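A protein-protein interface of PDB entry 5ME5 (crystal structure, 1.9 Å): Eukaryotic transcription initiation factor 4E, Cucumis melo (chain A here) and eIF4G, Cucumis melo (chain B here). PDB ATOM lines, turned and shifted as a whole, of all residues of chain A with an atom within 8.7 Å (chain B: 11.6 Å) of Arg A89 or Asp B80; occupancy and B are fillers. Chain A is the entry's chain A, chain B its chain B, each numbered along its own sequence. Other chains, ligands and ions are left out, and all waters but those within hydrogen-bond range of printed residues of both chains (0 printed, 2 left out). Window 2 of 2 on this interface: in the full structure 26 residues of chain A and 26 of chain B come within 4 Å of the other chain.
The side-chain amide nitrogen (ND2) of Asn A74 is in hydrogen-bond range of the backbone carbonyl oxygen (O) of Asp B80 (2.7 Å).
The side-chain hydroxyl (OG) of Ser B83 lies within hydrogen-bond range of the side-chain amide nitrogen (ND2) of Asn A74, 2.8 Å away.
The side-chain carboxylate (OD2) of Asp B80 lies within salt-bridge range of the guanidinium group (NE) of Arg A89 (3.7 Å).
The backbone carbonyl oxygen (O) of Phe A70 sits at hydrogen-bond distance from the backbone NH (N) of Ile A91, 2.8 Å away.
N of Phe A70 is in hydrogen-bond range of O of Tyr A92, at 2.9 Å.
N of Phe A72 sits at hydrogen-bond distance from O of Arg A89, 2.9 Å away.
The side-chain amide oxygen (OD1) of Asn A74 sits at hydrogen-bond distance from the backbone NH (N) of Ser A76, at 3.0 Å.
OG1 of Thr B78 is in hydrogen-bond range of OD1 of Asp B80 (2.6 Å).
CE2 of Phe A72 touches OG of Ser B83, at 3.7 Å.
CB of Leu B84 touches CE2 of Phe A72 (3.9 Å).
Phe B75 touches Ile A91.
Ile B81 touches Ile A91 (CG2 to CD1, 3.7 Å).
CG1 of Ile A91 touches CD2 of Leu B84, at 3.9 Å.
CD2 of Phe B75 touches CD1 of Tyr A92, at 3.4 Å.
CD1 of Leu A119 touches CD1 of Leu B84, 3.9 Å away.
No residue of chain B comes within 4 Å of Trp A71.
No residue of chain B comes within 4 Å of Asp A73.
Ser A87 touches none of the printed residues of chain B.
No residue of chain B comes within 4 Å of Ile A88.
Of the printed residues of chain B, Arg A89 touches Asp B80.
Pro A90 touches none of the printed residues of chain B.
Of the printed residues of chain B, Tyr A92 touches Phe B75.
Of the printed residues of chain A, Phe B75 touches Ile A91 and Tyr A92.
Ser B79 touches none of the printed residues of chain A.
Of chain A, only Asn A74 and Arg A89 come within 4 Å of Asp B80.
Printed residues of chain A within 4 Å of Ile B81: Ile A91 (3.7 Å).
Printed residues of chain A within 4 Å of Ser B83: Phe A72 (3.7 Å) and Asn A74 (2.8 Å).
Printed residues of chain A within 4 Å of Leu B84: Phe A72, Ile A91 and Leu A119.
The nearest residue of chain B that does not touch Arg A89 is Ile B81 (5.1 Å).
Of the 11 printed residues of chain B, 5 touch a printed residue of chain A.
Printed residues of chain B that touch a printed residue of chain A: Phe B75, Asp B80, Ile B81, Ser B83 and Leu B84.
Hydrophobic or aromatic side chains of chain B within 4 Å of the printed part of chain A: Phe B75, Ile B81 and Leu B84.
Hydrophobic or aromatic side chains of chain A that line the printed part of chain B: Phe A72, Ile A91, Tyr A92 and Leu A119.
Along chain A the printed residues that touch a printed residue of chain B span positions 72 to 119.
Among the printed residues, 10 pairs touch across the chains.
Among the printed residues, Asp or Glu carboxylates within 4 Å of a Lys or Arg side-chain nitrogen of the other chain: Arg A89 with Asp B80 (3.7 Å).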
ATOM      1  N   THR A  69      21.731  -6.581  28.879  1.00  0.00           N
ATOM      2  CA  THR A  69      21.007  -6.401  27.625  1.00  0.00           C
ATOM      3  C   THR A  69      20.087  -7.593  27.400  1.00  0.00           C
ATOM      4  O   THR A  69      20.535  -8.743  27.455  1.00  0.00           O
ATOM      5  CB  THR A  69      21.993  -6.247  26.465  1.00  0.00           C
ATOM      6  OG1 THR A  69      22.855  -5.130  26.724  1.00  0.00           O
ATOM      7  CG2 THR A  69      21.265  -6.029  25.146  1.00  0.00           C
ATOM      8  N   PHE A  70      18.795  -7.332  27.193  1.00  0.00           N
ATOM      9  CA  PHE A  70      17.908  -8.383  26.706  1.00  0.00           C
ATOM     10  C   PHE A  70      18.123  -8.571  25.212  1.00  0.00           C
ATOM     11  O   PHE A  70      18.259  -7.596  24.473  1.00  0.00           O
ATOM     12  CB  PHE A  70      16.429  -8.044  26.961  1.00  0.00           C
ATOM     13  CG  PHE A  70      15.987  -8.262  28.388  1.00  0.00           C
ATOM     14  CD1 PHE A  70      15.946  -9.537  28.933  1.00  0.00           C
ATOM     15  CD2 PHE A  70      15.614  -7.182  29.172  1.00  0.00           C
ATOM     16  CE1 PHE A  70      15.533  -9.739  30.268  1.00  0.00           C
ATOM     17  CE2 PHE A  70      15.210  -7.362  30.491  1.00  0.00           C
ATOM     18  CZ  PHE A  70      15.166  -8.638  31.040  1.00  0.00           C
ATOM     19  N   TRP A  71      18.146  -9.832  24.765  1.00  0.00           N
ATOM     20  CA  TRP A  71      18.164 -10.161  23.345  1.00  0.00           C
ATOM     21  C   TRP A  71      17.042 -11.145  23.057  1.00  0.00           C
ATOM     22  O   TRP A  71      16.637 -11.912  23.934  1.00  0.00           O
ATOM     23  CB  TRP A  71      19.474 -10.811  22.884  1.00  0.00           C
ATOM     24  CG  TRP A  71      20.736 -10.083  23.210  1.00  0.00           C
ATOM     25  CD1 TRP A  71      21.247  -9.837  24.445  1.00  0.00           C
ATOM     26  CD2 TRP A  71      21.678  -9.562  22.270  1.00  0.00           C
ATOM     27  NE1 TRP A  71      22.456  -9.179  24.335  1.00  0.00           N
ATOM     28  CE2 TRP A  71      22.734  -8.995  23.005  1.00  0.00           C
ATOM     29  CE3 TRP A  71      21.726  -9.517  20.873  1.00  0.00           C
ATOM     30  CZ2 TRP A  71      23.830  -8.382  22.390  1.00  0.00           C
ATOM     31  CZ3 TRP A  71      22.812  -8.927  20.269  1.00  0.00           C
ATOM     32  CH2 TRP A  71      23.846  -8.356  21.027  1.00  0.00           C
ATOM     33  N   PHE A  72      16.559 -11.139  21.815  1.00  0.00           N
ATOM     34  CA  PHE A  72      15.394 -11.943  21.461  1.00  0.00           C
ATOM     35  C   PHE A  72      15.608 -12.589  20.101  1.00  0.00           C
ATOM     36  O   PHE A  72      16.070 -11.936  19.163  1.00  0.00           O
ATOM     37  CB  PHE A  72      14.126 -11.072  21.448  1.00  0.00           C
ATOM     38  CG  PHE A  72      12.854 -11.839  21.222  1.00  0.00           C
ATOM     39  CD1 PHE A  72      12.528 -12.915  22.027  1.00  0.00           C
ATOM     40  CD2 PHE A  72      11.961 -11.451  20.238  1.00  0.00           C
ATOM     41  CE1 PHE A  72      11.342 -13.616  21.842  1.00  0.00           C
ATOM     42  CE2 PHE A  72      10.769 -12.143  20.050  1.00  0.00           C
ATOM     43  CZ  PHE A  72      10.464 -13.229  20.853  1.00  0.00           C
ATOM     44  N   ASP A  73      15.274 -13.868  19.996  1.00  0.00           N
ATOM     45  CA  ASP A  73      15.339 -14.591  18.728  1.00  0.00           C
ATOM     46  C   ASP A  73      13.916 -15.000  18.370  1.00  0.00           C
ATOM     47  O   ASP A  73      13.392 -15.976  18.914  1.00  0.00           O
ATOM     48  CB  ASP A  73      16.271 -15.800  18.818  1.00  0.00           C
ATOM     49  CG  ASP A  73      16.708 -16.303  17.446  1.00  0.00           C
ATOM     50  OD1 ASP A  73      16.157 -15.817  16.438  1.00  0.00           O
ATOM     51  OD2 ASP A  73      17.604 -17.175  17.375  1.00  0.00           O
ATOM     52  N   ASN A  74      13.309 -14.243  17.461  1.00  0.00           N
ATOM     53  CA  ASN A  74      11.907 -14.413  17.095  1.00  0.00           C
ATOM     54  C   ASN A  74      11.746 -15.620  16.184  1.00  0.00           C
ATOM     55  O   ASN A  74      12.383 -15.674  15.125  1.00  0.00           O
ATOM     56  CB  ASN A  74      11.398 -13.152  16.390  1.00  0.00           C
ATOM     57  CG  ASN A  74       9.878 -13.091  16.297  1.00  0.00           C
ATOM     58  OD1 ASN A  74       9.214 -14.103  16.064  1.00  0.00           O
ATOM     59  ND2 ASN A  74       9.321 -11.893  16.473  1.00  0.00           N
ATOM     60  N   PRO A  75      10.895 -16.591  16.529  1.00  0.00           N
ATOM     61  CA  PRO A  75      10.775 -17.773  15.663  1.00  0.00           C
ATOM     62  C   PRO A  75      10.022 -17.494  14.371  1.00  0.00           C
ATOM     63  O   PRO A  75      10.393 -18.034  13.319  1.00  0.00           O
ATOM     64  CB  PRO A  75      10.043 -18.779  16.560  1.00  0.00           C
ATOM     65  CG  PRO A  75       9.212 -17.927  17.463  1.00  0.00           C
ATOM     66  CD  PRO A  75       9.981 -16.647  17.687  1.00  0.00           C
ATOM     67  N   SER A  76       8.988 -16.654  14.412  1.00  0.00           N
ATOM     68  CA  SER A  76       8.181 -16.354  13.228  1.00  0.00           C
ATOM     69  C   SER A  76       8.921 -15.446  12.246  1.00  0.00           C
ATOM     70  O   SER A  76       9.646 -15.918  11.362  1.00  0.00           O
ATOM     71  CB  SER A  76       6.859 -15.718  13.641  1.00  0.00           C
ATOM     72  N   SER A  87      19.371 -12.860  13.312  1.00  0.00           N
ATOM     73  CA  SER A  87      18.341 -13.568  14.067  1.00  0.00           C
ATOM     74  C   SER A  87      18.207 -13.064  15.499  1.00  0.00           C
ATOM     75  O   SER A  87      17.114 -12.694  15.919  1.00  0.00           O
ATOM     76  CB  SER A  87      18.633 -15.069  14.085  1.00  0.00           C
ATOM     77  OG  SER A  87      18.383 -15.649  12.818  1.00  0.00           O
ATOM     78  N   ILE A  88      19.308 -13.052  16.247  1.00  0.00           N
ATOM     79  CA  ILE A  88      19.296 -12.673  17.660  1.00  0.00           C
ATOM     80  C   ILE A  88      19.488 -11.162  17.743  1.00  0.00           C
ATOM     81  O   ILE A  88      20.575 -10.654  17.463  1.00  0.00           O
ATOM     82  CB  ILE A  88      20.375 -13.418  18.458  1.00  0.00           C
ATOM     83  CG1 ILE A  88      20.255 -14.925  18.258  1.00  0.00           C
ATOM     84  CG2 ILE A  88      20.261 -13.086  19.935  1.00  0.00           C
ATOM     85  CD1 ILE A  88      21.370 -15.739  18.936  1.00  0.00           C
ATOM     86  N   ARG A  89      18.437 -10.441  18.159  1.00  0.00           N
ATOM     87  CA  ARG A  89      18.385  -8.986  18.150  1.00  0.00           C
ATOM     88  C   ARG A  89      18.475  -8.426  19.562  1.00  0.00           C
ATOM     89  O   ARG A  89      17.783  -8.916  20.462  1.00  0.00           O
ATOM     90  CB  ARG A  89      17.072  -8.506  17.527  1.00  0.00           C
ATOM     91  CG  ARG A  89      16.501  -9.444  16.492  1.00  0.00           C
ATOM     92  CD  ARG A  89      16.812  -8.948  15.100  1.00  0.00           C
ATOM     93  NE  ARG A  89      16.860  -7.486  15.089  1.00  0.00           N
ATOM     94  CZ  ARG A  89      17.278  -6.759  14.055  1.00  0.00           C
ATOM     95  NH1 ARG A  89      17.682  -7.357  12.942  1.00  0.00           N
ATOM     96  NH2 ARG A  89      17.284  -5.437  14.134  1.00  0.00           N
ATOM     97  N   PRO A  90      19.258  -7.373  19.777  1.00  0.00           N
ATOM     98  CA  PRO A  90      19.264  -6.722  21.087  1.00  0.00           C
ATOM     99  C   PRO A  90      18.019  -5.866  21.247  1.00  0.00           C
ATOM    100  O   PRO A  90      17.588  -5.176  20.319  1.00  0.00           O
ATOM    101  CB  PRO A  90      20.538  -5.873  21.049  1.00  0.00           C
ATOM    102  CG  PRO A  90      20.665  -5.502  19.583  1.00  0.00           C
ATOM    103  CD  PRO A  90      20.158  -6.712  18.815  1.00  0.00           C
ATOM    104  N   ILE A  91      17.436  -5.932  22.439  1.00  0.00           N
ATOM    105  CA  ILE A  91      16.158  -5.296  22.740  1.00  0.00           C
ATOM    106  C   ILE A  91      16.345  -4.014  23.528  1.00  0.00           C
ATOM    107  O   ILE A  91      15.791  -2.969  23.182  1.00  0.00           O
ATOM    108  CB  ILE A  91      15.269  -6.292  23.515  1.00  0.00           C
ATOM    109  CG1 ILE A  91      15.059  -7.560  22.693  1.00  0.00           C
ATOM    110  CG2 ILE A  91      13.973  -5.665  23.910  1.00  0.00           C
ATOM    111  CD1 ILE A  91      14.565  -7.293  21.302  1.00  0.00           C
ATOM    112  N   TYR A  92      17.102  -4.089  24.615  1.00  0.00           N
ATOM    113  CA  TYR A  92      17.211  -2.997  25.569  1.00  0.00           C
ATOM    114  C   TYR A  92      18.349  -3.305  26.520  1.00  0.00           C
ATOM    115  O   TYR A  92      18.515  -4.457  26.937  1.00  0.00           O
ATOM    116  CB  TYR A  92      15.914  -2.818  26.367  1.00  0.00           C
ATOM    117  CG  TYR A  92      15.855  -1.501  27.102  1.00  0.00           C
ATOM    118  CD1 TYR A  92      15.468  -0.332  26.448  1.00  0.00           C
ATOM    119  CD2 TYR A  92      16.193  -1.419  28.443  1.00  0.00           C
ATOM    120  CE1 TYR A  92      15.407   0.889  27.131  1.00  0.00           C
ATOM    121  CE2 TYR A  92      16.142  -0.215  29.128  1.00  0.00           C
ATOM    122  CZ  TYR A  92      15.750   0.931  28.469  1.00  0.00           C
ATOM    123  OH  TYR A  92      15.708   2.121  29.161  1.00  0.00           O
ATOM    124  N   ASP A 118      13.730 -17.671  21.743  1.00  0.00           N
ATOM    125  CA  ASP A 118      14.813 -17.622  22.715  1.00  0.00           C
ATOM    126  C   ASP A 118      14.903 -16.206  23.259  1.00  0.00           C
ATOM    127  O   ASP A 118      14.954 -15.244  22.484  1.00  0.00           O
ATOM    128  CB  ASP A 118      16.157 -18.012  22.104  1.00  0.00           C
ATOM    129  CG  ASP A 118      16.122 -19.373  21.423  1.00  0.00           C
ATOM    130  OD1 ASP A 118      15.533 -20.314  21.988  1.00  0.00           O
ATOM    131  OD2 ASP A 118      16.693 -19.490  20.323  1.00  0.00           O
ATOM    132  N   LEU A 119      14.903 -16.077  24.582  1.00  0.00           N
ATOM    133  CA  LEU A 119      15.029 -14.778  25.238  1.00  0.00           C
ATOM    134  C   LEU A 119      16.297 -14.795  26.073  1.00  0.00           C
ATOM    135  O   LEU A 119      16.460 -15.667  26.934  1.00  0.00           O
ATOM    136  CB  LEU A 119      13.808 -14.476  26.118  1.00  0.00           C
ATOM    137  CG  LEU A 119      13.804 -13.156  26.886  1.00  0.00           C
ATOM    138  CD1 LEU A 119      13.893 -11.994  25.914  1.00  0.00           C
ATOM    139  CD2 LEU A 119      12.550 -13.062  27.745  1.00  0.00           C
ATOM    140  N   TYR A 120      17.168 -13.815  25.841  1.00  0.00           N
ATOM    141  CA  TYR A 120      18.498 -13.756  26.437  1.00  0.00           C
ATOM    142  C   TYR A 120      18.587 -12.561  27.369  1.00  0.00           C
ATOM    143  O   TYR A 120      17.977 -11.524  27.114  1.00  0.00           O
ATOM    144  CB  TYR A 120      19.588 -13.582  25.370  1.00  0.00           C
ATOM    145  CG  TYR A 120      19.710 -14.691  24.358  1.00  0.00           C
ATOM    146  CD1 TYR A 120      18.834 -14.778  23.280  1.00  0.00           C
ATOM    147  CD2 TYR A 120      20.740 -15.630  24.453  1.00  0.00           C
ATOM    148  CE1 TYR A 120      18.961 -15.798  22.337  1.00  0.00           C
ATOM    149  CE2 TYR A 120      20.870 -16.645  23.529  1.00  0.00           C
ATOM    150  CZ  TYR A 120      19.979 -16.726  22.471  1.00  0.00           C
ATOM    151  OH  TYR A 120      20.123 -17.743  21.549  1.00  0.00           O
ATOM    152  N   PRO A 128      25.567 -12.902  22.980  1.00  0.00           N
ATOM    153  CA  PRO A 128      25.386 -14.362  22.992  1.00  0.00           C
ATOM    154  C   PRO A 128      25.552 -14.955  21.596  1.00  0.00           C
ATOM    155  O   PRO A 128      24.645 -15.580  21.044  1.00  0.00           O
ATOM    156  CB  PRO A 128      23.962 -14.509  23.544  1.00  0.00           C
ATOM    157  CG  PRO A 128      23.246 -13.298  23.050  1.00  0.00           C
ATOM    158  CD  PRO A 128      24.282 -12.183  23.111  1.00  0.00           C
ATOM    159  N   LYS A 129      26.736 -14.755  21.014  1.00  0.00           N
ATOM    160  CA  LYS A 129      27.001 -15.088  19.615  1.00  0.00           C
ATOM    161  C   LYS A 129      28.445 -15.549  19.466  1.00  0.00           C
ATOM    162  O   LYS A 129      29.246 -15.458  20.399  1.00  0.00           O
ATOM    163  CB  LYS A 129      26.757 -13.888  18.692  1.00  0.00           C
ATOM    164  CG  LYS A 129      25.305 -13.503  18.496  1.00  0.00           C
ATOM    165  CD  LYS A 129      25.169 -12.325  17.537  1.00  0.00           C
ATOM    166  CE  LYS A 129      23.717 -11.925  17.377  1.00  0.00           C
ATOM    167  NZ  LYS A 129      23.520 -10.848  16.366  1.00  0.00           N
ATOM    168  N   PHE B  75      12.601   2.847  25.119  1.00  0.00           N
ATOM    169  CA  PHE B  75      12.460   1.471  24.666  1.00  0.00           C
ATOM    170  C   PHE B  75      11.704   1.479  23.341  1.00  0.00           C
ATOM    171  O   PHE B  75      10.529   1.864  23.293  1.00  0.00           O
ATOM    172  CB  PHE B  75      11.722   0.637  25.719  1.00  0.00           C
ATOM    173  CG  PHE B  75      11.652  -0.826  25.404  1.00  0.00           C
ATOM    174  CD1 PHE B  75      10.857  -1.301  24.363  1.00  0.00           C
ATOM    175  CD2 PHE B  75      12.358  -1.741  26.171  1.00  0.00           C
ATOM    176  CE1 PHE B  75      10.795  -2.648  24.082  1.00  0.00           C
ATOM    177  CE2 PHE B  75      12.291  -3.079  25.900  1.00  0.00           C
ATOM    178  CZ  PHE B  75      11.511  -3.542  24.857  1.00  0.00           C
ATOM    179  N   GLU B  76      12.361   1.038  22.276  1.00  0.00           N
ATOM    180  CA  GLU B  76      11.750   1.025  20.952  1.00  0.00           C
ATOM    181  C   GLU B  76      11.102  -0.331  20.692  1.00  0.00           C
ATOM    182  O   GLU B  76      11.783  -1.361  20.704  1.00  0.00           O
ATOM    183  CB  GLU B  76      12.795   1.337  19.880  1.00  0.00           C
ATOM    184  CG  GLU B  76      12.194   1.551  18.506  1.00  0.00           C
ATOM    185  CD  GLU B  76      13.236   1.522  17.396  1.00  0.00           C
ATOM    186  OE1 GLU B  76      14.422   1.254  17.700  1.00  0.00           O
ATOM    187  OE2 GLU B  76      12.860   1.769  16.226  1.00  0.00           O
ATOM    188  N   VAL B  77       9.793  -0.337  20.450  1.00  0.00           N
ATOM    189  CA  VAL B  77       9.073  -1.555  20.092  1.00  0.00           C
ATOM    190  C   VAL B  77       8.980  -1.594  18.569  1.00  0.00           C
ATOM    191  O   VAL B  77       8.121  -0.943  17.967  1.00  0.00           O
ATOM    192  CB  VAL B  77       7.688  -1.627  20.740  1.00  0.00           C
ATOM    193  CG1 VAL B  77       7.069  -2.986  20.446  1.00  0.00           C
ATOM    194  CG2 VAL B  77       7.761  -1.396  22.245  1.00  0.00           C
ATOM    195  N   THR B  78       9.858  -2.360  17.938  1.00  0.00           N
ATOM    196  CA  THR B  78       9.803  -2.525  16.494  1.00  0.00           C
ATOM    197  C   THR B  78       8.866  -3.674  16.152  1.00  0.00           C
ATOM    198  O   THR B  78       8.524  -4.509  16.996  1.00  0.00           O
ATOM    199  CB  THR B  78      11.187  -2.794  15.902  1.00  0.00           C
ATOM    200  OG1 THR B  78      11.816  -3.848  16.636  1.00  0.00           O
ATOM    201  CG2 THR B  78      12.062  -1.543  15.959  1.00  0.00           C
ATOM    202  N   SER B  79       8.458  -3.710  14.887  1.00  0.00           N
ATOM    203  CA  SER B  79       7.471  -4.694  14.467  1.00  0.00           C
ATOM    204  C   SER B  79       7.967  -6.106  14.720  1.00  0.00           C
ATOM    205  O   SER B  79       7.222  -6.954  15.217  1.00  0.00           O
ATOM    206  CB  SER B  79       7.129  -4.485  12.994  1.00  0.00           C
ATOM    207  OG  SER B  79       6.435  -3.263  12.842  1.00  0.00           O
ATOM    208  N   ASP B  80       9.238  -6.362  14.433  1.00  0.00           N
ATOM    209  CA  ASP B  80       9.800  -7.695  14.583  1.00  0.00           C
ATOM    210  C   ASP B  80       9.887  -8.160  16.032  1.00  0.00           C
ATOM    211  O   ASP B  80      10.163  -9.344  16.262  1.00  0.00           O
ATOM    212  CB  ASP B  80      11.190  -7.740  13.955  1.00  0.00           C
ATOM    213  CG  ASP B  80      12.205  -6.954  14.751  1.00  0.00           C
ATOM    214  OD1 ASP B  80      12.011  -5.734  14.925  1.00  0.00           O
ATOM    215  OD2 ASP B  80      13.193  -7.557  15.214  1.00  0.00           O
ATOM    216  N   ILE B  81       9.690  -7.277  17.014  1.00  0.00           N
ATOM    217  CA  ILE B  81       9.698  -7.704  18.407  1.00  0.00           C
ATOM    218  C   ILE B  81       8.358  -7.473  19.086  1.00  0.00           C
ATOM    219  O   ILE B  81       8.263  -7.597  20.308  1.00  0.00           O
ATOM    220  CB  ILE B  81      10.837  -7.040  19.205  1.00  0.00           C
ATOM    221  CG1 ILE B  81      10.556  -5.554  19.435  1.00  0.00           C
ATOM    222  CG2 ILE B  81      12.182  -7.289  18.528  1.00  0.00           C
ATOM    223  CD1 ILE B  81      11.460  -4.937  20.472  1.00  0.00           C
ATOM    224  N   GLU B  82       7.312  -7.143  18.320  1.00  0.00           N
ATOM    225  CA  GLU B  82       5.993  -6.990  18.920  1.00  0.00           C
ATOM    226  C   GLU B  82       5.554  -8.270  19.622  1.00  0.00           C
ATOM    227  O   GLU B  82       4.875  -8.209  20.654  1.00  0.00           O
ATOM    228  CB  GLU B  82       4.971  -6.577  17.859  1.00  0.00           C
ATOM    229  CG  GLU B  82       5.016  -5.094  17.491  1.00  0.00           C
ATOM    230  CD  GLU B  82       3.944  -4.696  16.472  1.00  0.00           C
ATOM    231  OE1 GLU B  82       4.229  -3.857  15.585  1.00  0.00           O
ATOM    232  OE2 GLU B  82       2.811  -5.218  16.561  1.00  0.00           O
ATOM    233  N   SER B  83       5.966  -9.432  19.108  1.00  0.00           N
ATOM    234  CA  SER B  83       5.620 -10.717  19.706  1.00  0.00           C
ATOM    235  C   SER B  83       6.284 -10.940  21.060  1.00  0.00           C
ATOM    236  O   SER B  83       5.880 -11.863  21.776  1.00  0.00           O
ATOM    237  CB  SER B  83       5.997 -11.857  18.757  1.00  0.00           C
ATOM    238  OG  SER B  83       7.399 -11.913  18.553  1.00  0.00           O
ATOM    239  N   LEU B  84       7.284 -10.126  21.423  1.00  0.00           N
ATOM    240  CA  LEU B  84       7.911 -10.222  22.736  1.00  0.00           C
ATOM    241  C   LEU B  84       7.141  -9.462  23.812  1.00  0.00           C
ATOM    242  O   LEU B  84       7.230  -9.820  24.992  1.00  0.00           O
ATOM    243  CB  LEU B  84       9.346  -9.696  22.667  1.00  0.00           C
ATOM    244  CG  LEU B  84      10.175  -9.587  23.960  1.00  0.00           C
ATOM    245  CD1 LEU B  84      10.309 -10.951  24.690  1.00  0.00           C
ATOM    246  CD2 LEU B  84      11.550  -8.995  23.647  1.00  0.00           C
ATOM    247  N   MET B  85       6.383  -8.427  23.432  1.00  0.00           N
ATOM    248  CA  MET B  85       5.787  -7.508  24.396  1.00  0.00           C
ATOM    249  C   MET B  85       4.605  -8.142  25.126  1.00  0.00           C
ATOM    250  O   MET B  85       3.856  -8.952  24.566  1.00  0.00           O
ATOM    251  CB  MET B  85       5.325  -6.225  23.687  1.00  0.00           C
ATOM    252  CG  MET B  85       6.424  -5.544  22.893  1.00  0.00           C
ATOM    253  SD  MET B  85       7.969  -5.434  23.826  1.00  0.00           S
ATOM    254  CE  MET B  85       7.547  -4.199  25.043  1.00  0.00           C
